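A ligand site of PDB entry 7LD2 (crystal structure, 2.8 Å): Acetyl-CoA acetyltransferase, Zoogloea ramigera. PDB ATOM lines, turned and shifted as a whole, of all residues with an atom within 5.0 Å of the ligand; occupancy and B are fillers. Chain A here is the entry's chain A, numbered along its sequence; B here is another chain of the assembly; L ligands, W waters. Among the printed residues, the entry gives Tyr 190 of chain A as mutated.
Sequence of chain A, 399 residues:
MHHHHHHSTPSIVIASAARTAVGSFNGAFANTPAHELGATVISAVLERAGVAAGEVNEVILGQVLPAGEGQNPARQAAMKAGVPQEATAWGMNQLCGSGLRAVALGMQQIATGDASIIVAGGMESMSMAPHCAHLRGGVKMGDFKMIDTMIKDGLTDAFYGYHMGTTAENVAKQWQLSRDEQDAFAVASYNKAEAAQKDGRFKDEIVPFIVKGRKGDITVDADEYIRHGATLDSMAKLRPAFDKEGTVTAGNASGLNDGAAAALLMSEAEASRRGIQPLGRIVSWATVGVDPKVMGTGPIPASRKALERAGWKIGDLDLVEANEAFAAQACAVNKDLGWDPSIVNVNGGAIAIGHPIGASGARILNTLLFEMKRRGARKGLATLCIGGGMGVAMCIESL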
ATOM      1  N   SCY A  96      19.672  34.673   5.477  1.00  0.00           N
ATOM      2  CA  SCY A  96      20.777  34.442   6.404  1.00  0.00           C
ATOM      3  CB  SCY A  96      21.980  33.866   5.678  1.00  0.00           C
ATOM      4  SG  SCY A  96      21.644  32.255   4.998  1.00  0.00           S
ATOM      5  CD  SCY A  96      21.041  32.501   3.422  1.00  0.00           C
ATOM      6  OCD SCY A  96      21.252  33.465   2.674  1.00  0.00           O
ATOM      7  CE  SCY A  96      20.171  31.361   3.012  1.00  0.00           C
ATOM      8  C   SCY A  96      21.292  35.701   7.197  1.00  0.00           C
ATOM      9  O   SCY A  96      21.856  35.518   8.311  1.00  0.00           O
ATOM     10  N   LEU A 155      16.654  27.537   1.526  1.00  0.00           N
ATOM     11  CA  LEU A 155      17.888  27.015   0.963  1.00  0.00           C
ATOM     12  C   LEU A 155      17.898  26.914  -0.559  1.00  0.00           C
ATOM     13  O   LEU A 155      18.942  26.572  -1.123  1.00  0.00           O
ATOM     14  CB  LEU A 155      18.196  25.632   1.551  1.00  0.00           C
ATOM     15  CG  LEU A 155      18.252  25.549   3.078  1.00  0.00           C
ATOM     16  CD1 LEU A 155      18.518  24.124   3.523  1.00  0.00           C
ATOM     17  CD2 LEU A 155      19.298  26.500   3.624  1.00  0.00           C
ATOM     18  N   HIS A 163      20.225  24.610  -5.006  1.00  0.00           N
ATOM     19  CA  HIS A 163      20.530  24.857  -3.612  1.00  0.00           C
ATOM     20  C   HIS A 163      21.586  25.950  -3.474  1.00  0.00           C
ATOM     21  O   HIS A 163      22.266  26.315  -4.437  1.00  0.00           O
ATOM     22  CB  HIS A 163      21.019  23.568  -2.940  1.00  0.00           C
ATOM     23  CG  HIS A 163      20.910  23.572  -1.442  1.00  0.00           C
ATOM     24  ND1 HIS A 163      21.875  24.106  -0.624  1.00  0.00           N
ATOM     25  CD2 HIS A 163      19.954  23.076  -0.622  1.00  0.00           C
ATOM     26  CE1 HIS A 163      21.523  23.961   0.638  1.00  0.00           C
ATOM     27  NE2 HIS A 163      20.355  23.335   0.668  1.00  0.00           N
ATOM     28  N   MET A 164      21.716  26.471  -2.254  1.00  0.00           N
ATOM     29  CA  MET A 164      22.781  27.431  -1.964  1.00  0.00           C
ATOM     30  C   MET A 164      24.155  26.800  -2.113  1.00  0.00           C
ATOM     31  O   MET A 164      25.126  27.519  -2.357  1.00  0.00           O
ATOM     32  CB  MET A 164      22.617  27.995  -0.559  1.00  0.00           C
ATOM     33  CG  MET A 164      21.364  28.837  -0.346  1.00  0.00           C
ATOM     34  SD  MET A 164      21.472  30.494  -1.085  1.00  0.00           S
ATOM     35  CE  MET A 164      20.723  30.212  -2.691  1.00  0.00           C
ATOM     36  N   TYR A 190      36.894  23.525  12.419  1.00  0.00           N
ATOM     37  CA  TYR A 190      36.502  22.564  13.434  1.00  0.00           C
ATOM     38  C   TYR A 190      37.453  22.621  14.626  1.00  0.00           C
ATOM     39  O   TYR A 190      37.012  22.612  15.785  1.00  0.00           O
ATOM     40  CB  TYR A 190      36.490  21.150  12.849  1.00  0.00           C
ATOM     41  CG  TYR A 190      35.352  20.875  11.874  1.00  0.00           C
ATOM     42  CD1 TYR A 190      34.035  20.956  12.274  1.00  0.00           C
ATOM     43  CD2 TYR A 190      35.618  20.491  10.563  1.00  0.00           C
ATOM     44  CE1 TYR A 190      33.000  20.697  11.393  1.00  0.00           C
ATOM     45  CE2 TYR A 190      34.600  20.226   9.675  1.00  0.00           C
ATOM     46  CZ  TYR A 190      33.292  20.331  10.102  1.00  0.00           C
ATOM     47  OH  TYR A 190      32.271  20.057   9.212  1.00  0.00           O
ATOM     48  N   TYR A 225      26.660  20.781  17.858  1.00  0.00           N
ATOM     49  CA  TYR A 225      27.078  20.522  16.485  1.00  0.00           C
ATOM     50  C   TYR A 225      28.583  20.489  16.328  1.00  0.00           C
ATOM     51  O   TYR A 225      29.083  19.968  15.326  1.00  0.00           O
ATOM     52  CB  TYR A 225      26.477  21.579  15.551  1.00  0.00           C
ATOM     53  CG  TYR A 225      26.624  21.243  14.084  1.00  0.00           C
ATOM     54  CD1 TYR A 225      25.866  20.230  13.516  1.00  0.00           C
ATOM     55  CD2 TYR A 225      27.513  21.932  13.273  1.00  0.00           C
ATOM     56  CE1 TYR A 225      25.993  19.925  12.164  1.00  0.00           C
ATOM     57  CE2 TYR A 225      27.646  21.633  11.933  1.00  0.00           C
ATOM     58  CZ  TYR A 225      26.880  20.629  11.391  1.00  0.00           C
ATOM     59  OH  TYR A 225      27.010  20.320  10.049  1.00  0.00           O
ATOM     60  N   ARG A 227      31.956  19.071  16.387  1.00  0.00           N
ATOM     61  CA  ARG A 227      32.489  17.707  16.448  1.00  0.00           C
ATOM     62  C   ARG A 227      33.889  17.713  17.052  1.00  0.00           C
ATOM     63  O   ARG A 227      34.688  18.618  16.792  1.00  0.00           O
ATOM     64  CB  ARG A 227      32.511  17.067  15.063  1.00  0.00           C
ATOM     65  CG  ARG A 227      33.363  17.792  14.033  1.00  0.00           C
ATOM     66  CD  ARG A 227      32.996  17.388  12.619  1.00  0.00           C
ATOM     67  NE  ARG A 227      32.992  15.938  12.425  1.00  0.00           N
ATOM     68  CZ  ARG A 227      31.888  15.201  12.266  1.00  0.00           C
ATOM     69  NH1 ARG A 227      30.697  15.781  12.274  1.00  0.00           N
ATOM     70  NH2 ARG A 227      31.986  13.890  12.098  1.00  0.00           N
ATOM     71  N   SER A 234      39.003  11.343   6.979  1.00  0.00           N
ATOM     72  CA  SER A 234      37.575  11.096   6.766  1.00  0.00           C
ATOM     73  C   SER A 234      36.890  12.288   6.112  1.00  0.00           C
ATOM     74  O   SER A 234      35.784  12.142   5.589  1.00  0.00           O
ATOM     75  CB  SER A 234      36.890  10.760   8.092  1.00  0.00           C
ATOM     76  OG  SER A 234      36.791  11.908   8.921  1.00  0.00           O
ATOM     77  N   MET A 235      37.534  13.458   6.131  1.00  0.00           N
ATOM     78  CA  MET A 235      36.960  14.635   5.482  1.00  0.00           C
ATOM     79  C   MET A 235      37.010  14.516   3.964  1.00  0.00           C
ATOM     80  O   MET A 235      36.103  14.971   3.269  1.00  0.00           O
ATOM     81  CB  MET A 235      37.695  15.889   5.940  1.00  0.00           C
ATOM     82  CG  MET A 235      36.999  17.189   5.601  1.00  0.00           C
ATOM     83  SD  MET A 235      35.656  17.532   6.744  1.00  0.00           S
ATOM     84  CE  MET A 235      36.533  17.482   8.298  1.00  0.00           C
ATOM     85  N   LEU A 238      34.320  12.013   2.060  1.00  0.00           N
ATOM     86  CA  LEU A 238      32.935  12.433   1.845  1.00  0.00           C
ATOM     87  C   LEU A 238      32.707  12.807   0.381  1.00  0.00           C
ATOM     88  O   LEU A 238      33.589  13.360  -0.287  1.00  0.00           O
ATOM     89  CB  LEU A 238      32.604  13.621   2.740  1.00  0.00           C
ATOM     90  CG  LEU A 238      32.767  13.409   4.246  1.00  0.00           C
ATOM     91  CD1 LEU A 238      32.525  14.698   5.002  1.00  0.00           C
ATOM     92  CD2 LEU A 238      31.807  12.332   4.720  1.00  0.00           C
ATOM     93  N   ALA A 241      27.661  16.946  -1.932  1.00  0.00           N
ATOM     94  CA  ALA A 241      26.251  16.898  -1.569  1.00  0.00           C
ATOM     95  C   ALA A 241      25.348  17.649  -2.541  1.00  0.00           C
ATOM     96  O   ALA A 241      24.127  17.643  -2.355  1.00  0.00           O
ATOM     97  CB  ALA A 241      26.058  17.474  -0.162  1.00  0.00           C
ATOM     98  N   PHE A 242      25.909  18.288  -3.573  1.00  0.00           N
ATOM     99  CA  PHE A 242      25.084  19.055  -4.510  1.00  0.00           C
ATOM    100  C   PHE A 242      25.383  18.659  -5.946  1.00  0.00           C
ATOM    101  O   PHE A 242      24.535  18.048  -6.617  1.00  0.00           O
ATOM    102  CB  PHE A 242      25.307  20.551  -4.294  1.00  0.00           C
ATOM    103  CG  PHE A 242      25.150  20.977  -2.872  1.00  0.00           C
ATOM    104  CD1 PHE A 242      23.892  21.122  -2.305  1.00  0.00           C
ATOM    105  CD2 PHE A 242      26.263  21.243  -2.079  1.00  0.00           C
ATOM    106  CE1 PHE A 242      23.745  21.509  -0.986  1.00  0.00           C
ATOM    107  CE2 PHE A 242      26.128  21.636  -0.763  1.00  0.00           C
ATOM    108  CZ  PHE A 242      24.866  21.766  -0.222  1.00  0.00           C
ATOM    109  N   THR A 249      31.065  19.612   0.020  1.00  0.00           N
ATOM    110  CA  THR A 249      30.532  18.442   0.713  1.00  0.00           C
ATOM    111  C   THR A 249      29.884  18.878   2.020  1.00  0.00           C
ATOM    112  O   THR A 249      29.879  20.057   2.379  1.00  0.00           O
ATOM    113  CB  THR A 249      31.635  17.406   0.968  1.00  0.00           C
ATOM    114  OG1 THR A 249      32.592  17.943   1.899  1.00  0.00           O
ATOM    115  CG2 THR A 249      32.342  17.052  -0.319  1.00  0.00           C
ATOM    116  N   ALA A 250      29.326  17.901   2.741  1.00  0.00           N
ATOM    117  CA  ALA A 250      28.744  18.199   4.047  1.00  0.00           C
ATOM    118  C   ALA A 250      29.796  18.555   5.075  1.00  0.00           C
ATOM    119  O   ALA A 250      29.454  19.110   6.126  1.00  0.00           O
ATOM    120  CB  ALA A 250      27.911  17.010   4.532  1.00  0.00           C
ATOM    121  N   GLY A 251      31.058  18.250   4.806  1.00  0.00           N
ATOM    122  CA  GLY A 251      32.138  18.561   5.723  1.00  0.00           C
ATOM    123  C   GLY A 251      32.638  19.978   5.583  1.00  0.00           C
ATOM    124  O   GLY A 251      32.887  20.656   6.587  1.00  0.00           O
ATOM    125  N   ALA A 253      30.895  22.423   4.315  1.00  0.00           N
ATOM    126  CA  ALA A 253      29.760  23.326   4.302  1.00  0.00           C
ATOM    127  C   ALA A 253      29.150  23.397   5.696  1.00  0.00           C
ATOM    128  O   ALA A 253      29.390  22.553   6.550  1.00  0.00           O
ATOM    129  CB  ALA A 253      28.689  22.885   3.296  1.00  0.00           C
ATOM    130  N   SER A 254      28.341  24.437   5.911  1.00  0.00           N
ATOM    131  CA  SER A 254      27.634  24.586   7.174  1.00  0.00           C
ATOM    132  C   SER A 254      26.533  23.532   7.272  1.00  0.00           C
ATOM    133  O   SER A 254      26.346  22.694   6.382  1.00  0.00           O
ATOM    134  CB  SER A 254      27.062  25.995   7.304  1.00  0.00           C
ATOM    135  OG  SER A 254      26.237  26.330   6.203  1.00  0.00           O
ATOM    136  N   GLY A 255      25.787  23.576   8.369  1.00  0.00           N
ATOM    137  CA  GLY A 255      24.720  22.625   8.600  1.00  0.00           C
ATOM    138  C   GLY A 255      23.408  23.327   8.918  1.00  0.00           C
ATOM    139  O   GLY A 255      23.347  24.545   9.087  1.00  0.00           O
ATOM    140  N   LEU A 256      22.354  22.512   8.991  1.00  0.00           N
ATOM    141  CA  LEU A 256      21.032  22.982   9.389  1.00  0.00           C
ATOM    142  C   LEU A 256      20.942  22.920  10.904  1.00  0.00           C
ATOM    143  O   LEU A 256      21.204  21.883  11.512  1.00  0.00           O
ATOM    144  CB  LEU A 256      19.958  22.107   8.746  1.00  0.00           C
ATOM    145  CG  LEU A 256      20.232  21.667   7.314  1.00  0.00           C
ATOM    146  CD1 LEU A 256      19.157  20.716   6.833  1.00  0.00           C
ATOM    147  CD2 LEU A 256      20.333  22.874   6.407  1.00  0.00           C
ATOM    148  N   MET A 295      26.198  34.304  -4.638  1.00  0.00           N
ATOM    149  CA  MET A 295      25.765  34.973  -3.411  1.00  0.00           C
ATOM    150  C   MET A 295      26.809  34.889  -2.317  1.00  0.00           C
ATOM    151  O   MET A 295      26.733  35.645  -1.339  1.00  0.00           O
ATOM    152  CB  MET A 295      24.440  34.391  -2.932  1.00  0.00           C
ATOM    153  CG  MET A 295      24.537  32.959  -2.425  1.00  0.00           C
ATOM    154  SD  MET A 295      24.802  32.871  -0.646  1.00  0.00           S
ATOM    155  CE  MET A 295      25.142  31.123  -0.464  1.00  0.00           C
ATOM    156  N   ALA A 325      29.166  30.121   5.653  1.00  0.00           N
ATOM    157  CA  ALA A 325      28.109  29.333   5.033  1.00  0.00           C
ATOM    158  C   ALA A 325      28.676  28.166   4.247  1.00  0.00           C
ATOM    159  O   ALA A 325      28.146  27.046   4.296  1.00  0.00           O
ATOM    160  CB  ALA A 325      27.253  30.226   4.136  1.00  0.00           C
ATOM    161  N   PHE A 326      29.763  28.404   3.509  1.00  0.00           N
ATOM    162  CA  PHE A 326      30.465  27.355   2.786  1.00  0.00           C
ATOM    163  C   PHE A 326      31.959  27.654   2.820  1.00  0.00           C
ATOM    164  O   PHE A 326      32.370  28.814   2.887  1.00  0.00           O
ATOM    165  CB  PHE A 326      29.986  27.237   1.336  1.00  0.00           C
ATOM    166  CG  PHE A 326      28.526  26.933   1.202  1.00  0.00           C
ATOM    167  CD1 PHE A 326      28.085  25.616   1.213  1.00  0.00           C
ATOM    168  CD2 PHE A 326      27.598  27.939   1.059  1.00  0.00           C
ATOM    169  CE1 PHE A 326      26.741  25.318   1.078  1.00  0.00           C
ATOM    170  CE2 PHE A 326      26.249  27.653   0.929  1.00  0.00           C
ATOM    171  CZ  PHE A 326      25.819  26.331   0.945  1.00  0.00           C
ATOM    172  N   HIS A 355      24.578  26.830  11.589  1.00  0.00           N
ATOM    173  CA  HIS A 355      24.061  27.963  10.819  1.00  0.00           C
ATOM    174  C   HIS A 355      22.548  27.989  10.855  1.00  0.00           C
ATOM    175  O   HIS A 355      21.882  27.565   9.902  1.00  0.00           O
ATOM    176  CB  HIS A 355      24.579  27.918   9.375  1.00  0.00           C
ATOM    177  CG  HIS A 355      24.239  29.135   8.577  1.00  0.00           C
ATOM    178  ND1 HIS A 355      24.668  30.397   8.926  1.00  0.00           N
ATOM    179  CD2 HIS A 355      23.518  29.278   7.445  1.00  0.00           C
ATOM    180  CE1 HIS A 355      24.222  31.268   8.046  1.00  0.00           C
ATOM    181  NE2 HIS A 355      23.519  30.620   7.130  1.00  0.00           N
ATOM    182  N   ILE A 357      19.605  30.040  10.023  1.00  0.00           N
ATOM    183  CA  ILE A 357      19.607  31.109   9.024  1.00  0.00           C
ATOM    184  C   ILE A 357      19.164  32.436   9.625  1.00  0.00           C
ATOM    185  O   ILE A 357      19.898  33.434   9.592  1.00  0.00           O
ATOM    186  CB  ILE A 357      18.756  30.717   7.799  1.00  0.00           C
ATOM    187  CG1 ILE A 357      17.471  30.006   8.234  1.00  0.00           C
ATOM    188  CG2 ILE A 357      19.544  29.817   6.867  1.00  0.00           C
ATOM    189  CD1 ILE A 357      16.648  29.479   7.076  1.00  0.00           C
ATOM    190  N   CYS A 385      26.930  36.330   4.270  1.00  0.00           N
ATOM    191  CA  CYS A 385      26.379  36.278   2.920  1.00  0.00           C
ATOM    192  C   CYS A 385      24.900  35.931   2.987  1.00  0.00           C
ATOM    193  O   CYS A 385      24.445  35.180   3.850  1.00  0.00           O
ATOM    194  CB  CYS A 385      27.133  35.257   2.058  1.00  0.00           C
ATOM    195  SG  CYS A 385      26.992  33.549   2.626  1.00  0.00           S
ATOM    196  N   MET B 141      14.357  15.417   5.671  1.00  0.00           N
ATOM    197  CA  MET B 141      14.651  16.553   4.822  1.00  0.00           C
ATOM    198  C   MET B 141      14.207  16.239   3.395  1.00  0.00           C
ATOM    199  O   MET B 141      14.268  15.085   2.961  1.00  0.00           O
ATOM    200  CB  MET B 141      16.144  16.906   4.863  1.00  0.00           C
ATOM    201  CG  MET B 141      16.556  18.073   3.997  1.00  0.00           C
ATOM    202  SD  MET B 141      18.323  18.414   4.179  1.00  0.00           S
ATOM    203  CE  MET B 141      19.011  16.829   3.689  1.00  0.00           C
HETATM  204  N1  LIG L   1      33.845  14.859   9.126  1.00  0.00           N
HETATM  205  C1  LIG L   1      33.506  13.625   8.780  1.00  0.00           C
HETATM  206  N2  LIG L   1      32.312  13.313   8.339  1.00  0.00           N
HETATM  207  C2  LIG L   1      31.371  14.241   8.229  1.00  0.00           C
HETATM  208  C3  LIG L   1      31.675  15.565   8.583  1.00  0.00           C
HETATM  209  C4  LIG L   1      32.971  15.854   9.039  1.00  0.00           C
HETATM  210  N3  LIG L   1      33.311  17.139   9.401  1.00  0.00           N
HETATM  211  N4  LIG L   1      30.565  16.300   8.363  1.00  0.00           N
HETATM  212  C5  LIG L   1      29.612  15.533   7.915  1.00  0.00           C
HETATM  213  N5  LIG L   1      30.065  14.248   7.808  1.00  0.00           N
HETATM  214  C6  LIG L   1      29.273  13.108   7.340  1.00  0.00           C
HETATM  215  C7  LIG L   1      28.098  12.831   8.302  1.00  0.00           C
HETATM  216  O1  LIG L   1      28.506  12.011   9.397  1.00  0.00           O
HETATM  217  C8  LIG L   1      27.155  12.074   7.337  1.00  0.00           C
HETATM  218  O2  LIG L   1      27.655  10.756   7.072  1.00  0.00           O
HETATM  219  P1  LIG L   1      26.663   9.669   7.719  1.00  0.00           P
HETATM  220  O3  LIG L   1      25.793   9.108   6.664  1.00  0.00           O
HETATM  221  O4  LIG L   1      27.515   8.481   8.386  1.00  0.00           O
HETATM  222  O5  LIG L   1      25.760  10.366   8.862  1.00  0.00           O
HETATM  223  C9  LIG L   1      27.287  12.959   6.093  1.00  0.00           C
HETATM  224  O6  LIG L   1      28.639  13.439   6.077  1.00  0.00           O
HETATM  225  C10 LIG L   1      26.332  14.155   6.164  1.00  0.00           C
HETATM  226  O7  LIG L   1      25.284  13.939   7.106  1.00  0.00           O
HETATM  227  P2  LIG L   1      24.944  15.360   7.794  1.00  0.00           P
HETATM  228  O8  LIG L   1      26.108  15.828   8.571  1.00  0.00           O
HETATM  229  O9  LIG L   1      23.719  15.158   8.818  1.00  0.00           O
HETATM  230  O10 LIG L   1      24.579  16.475   6.673  1.00  0.00           O
HETATM  231  P3  LIG L   1      23.147  16.220   5.952  1.00  0.00           P
HETATM  232  O11 LIG L   1      23.111  14.885   5.301  1.00  0.00           O
HETATM  233  O12 LIG L   1      21.953  16.334   7.038  1.00  0.00           O
HETATM  234  O13 LIG L   1      22.906  17.332   4.802  1.00  0.00           O
HETATM  235  C11 LIG L   1      23.765  19.399   3.896  1.00  0.00           C
HETATM  236  C12 LIG L   1      24.088  18.128   4.670  1.00  0.00           C
HETATM  237  C13 LIG L   1      25.033  19.942   3.235  1.00  0.00           C
HETATM  238  C14 LIG L   1      22.720  19.083   2.823  1.00  0.00           C
HETATM  239  C15 LIG L   1      23.205  20.448   4.871  1.00  0.00           C
HETATM  240  O14 LIG L   1      23.943  20.369   6.096  1.00  0.00           O
HETATM  241  C16 LIG L   1      23.333  21.848   4.327  1.00  0.00           C
HETATM  242  O15 LIG L   1      22.778  22.155   3.295  1.00  0.00           O
HETATM  243  N6  LIG L   1      24.051  22.767   5.009  1.00  0.00           N
HETATM  244  C17 LIG L   1      24.169  24.131   4.500  1.00  0.00           C
HETATM  245  C18 LIG L   1      23.009  24.988   4.997  1.00  0.00           C
HETATM  246  C19 LIG L   1      22.830  26.188   4.109  1.00  0.00           C
HETATM  247  O16 LIG L   1      22.734  26.047   2.905  1.00  0.00           O
HETATM  248  N7  LIG L   1      22.766  27.421   4.659  1.00  0.00           N
HETATM  249  C20 LIG L   1      22.591  28.618   3.835  1.00  0.00           C
HETATM  250  C21 LIG L   1      23.950  29.016   3.262  1.00  0.00           C
HETATM  251  S1  LIG L   1      23.911  30.756   2.751  1.00  0.00           S
HETATM  252  O   HOH W   1      23.640  16.936  11.775  1.00  0.00           O
HETATM  253  O   HOH W   2      21.390  16.211  10.662  1.00  0.00           O
HETATM  254  O   HOH W   3      20.087  21.029   2.079  1.00  0.00           O
HETATM  255  O   HOH W   4      22.548  18.846   8.860  1.00  0.00           O
HETATM  256  O   HOH W   5      28.312   9.615  10.600  1.00  0.00           O
HETATM  257  O   HOH W   6      25.443  18.689   9.091  1.00  0.00           O
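OH of Tyr 190 sits at hydrogen-bond distance from N3 of the ligand (3.1 Å).
SG of SCY 96 lies close to a sulfur (S1) of the ligand.
The backbone carbonyl oxygen (O) of Ser 254 lies within hydrogen-bond range of a nitrogen (N6) of the ligand (2.7 Å).
A nitrogen (N3) of the ligand sits close to the side-chain sulfur (SD) of Met 235 (3.6 Å).
The backbone NH (N) of Met 164 lies within hydrogen-bond range of the backbone carbonyl oxygen (O) of Leu 155 (3.0 Å).
The side-chain hydroxyl (OG) of Ser 254 sits at hydrogen-bond distance from the backbone carbonyl oxygen (O) of Ala 325 (2.8 Å).
SG of SCY 96 lies within hydrogen-bond range of NE2 of His 355, 3.3 Å away.
The backbone carbonyl oxygen (O) of Gly 251 is in hydrogen-bond range of the side-chain hydroxyl (OH) of Tyr 190 (2.8 Å).
The side-chain hydroxyl (OG1) of Thr 249 sits close to the backbone NH (N) of Gly 251.
A nitrogen (N3) of the ligand lies close to the guanidinium group (NE) of Arg 227 (3.3 Å).
Merely in contact with the ligand: Leu 155 (3.5 Å), His 163 (3.3 Å), Met 164 (3.98 Å), Ser 234 (3.7 Å), Leu 238 (3.5 Å), Phe 242 (3.9 Å), Ala 250 (3.6 Å), Gly 251 (3.8 Å), Gly 255 (3.5 Å), Leu 256 (3.7 Å), Met 295 (3.5 Å), Ala 325 (3.6 Å), Phe 326 (3.5 Å) and His 355 (3.4 Å).
Hydrophobic or aromatic side chains that line the ligand: Leu 155, His 163, Met 164, Tyr 190, Met 235, Leu 238, Phe 242, Ala 250, Leu 256, Met 295, Ala 325, Phe 326 and His 355.
Within 4 Å of the ligand: SCY 96, Leu 155, His 163, Met 164, Tyr 190, Arg 227, Ser 234, Met 235, Leu 238, Phe 242, Ala 250, Gly 251, Ser 254, Gly 255, Leu 256, Met 295, Ala 325, Phe 326 and His 355.
Water W6 lies within hydrogen-bond range of the side-chain hydroxyl of Tyr 225 and an oxygen (O8) of the ligand.
Water W3 lies within hydrogen-bond range of NE2 of His 163 (2.7 Å), O15 of the ligand (3.2 Å) and SD of Met 141 of chain B (3.8 Å).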
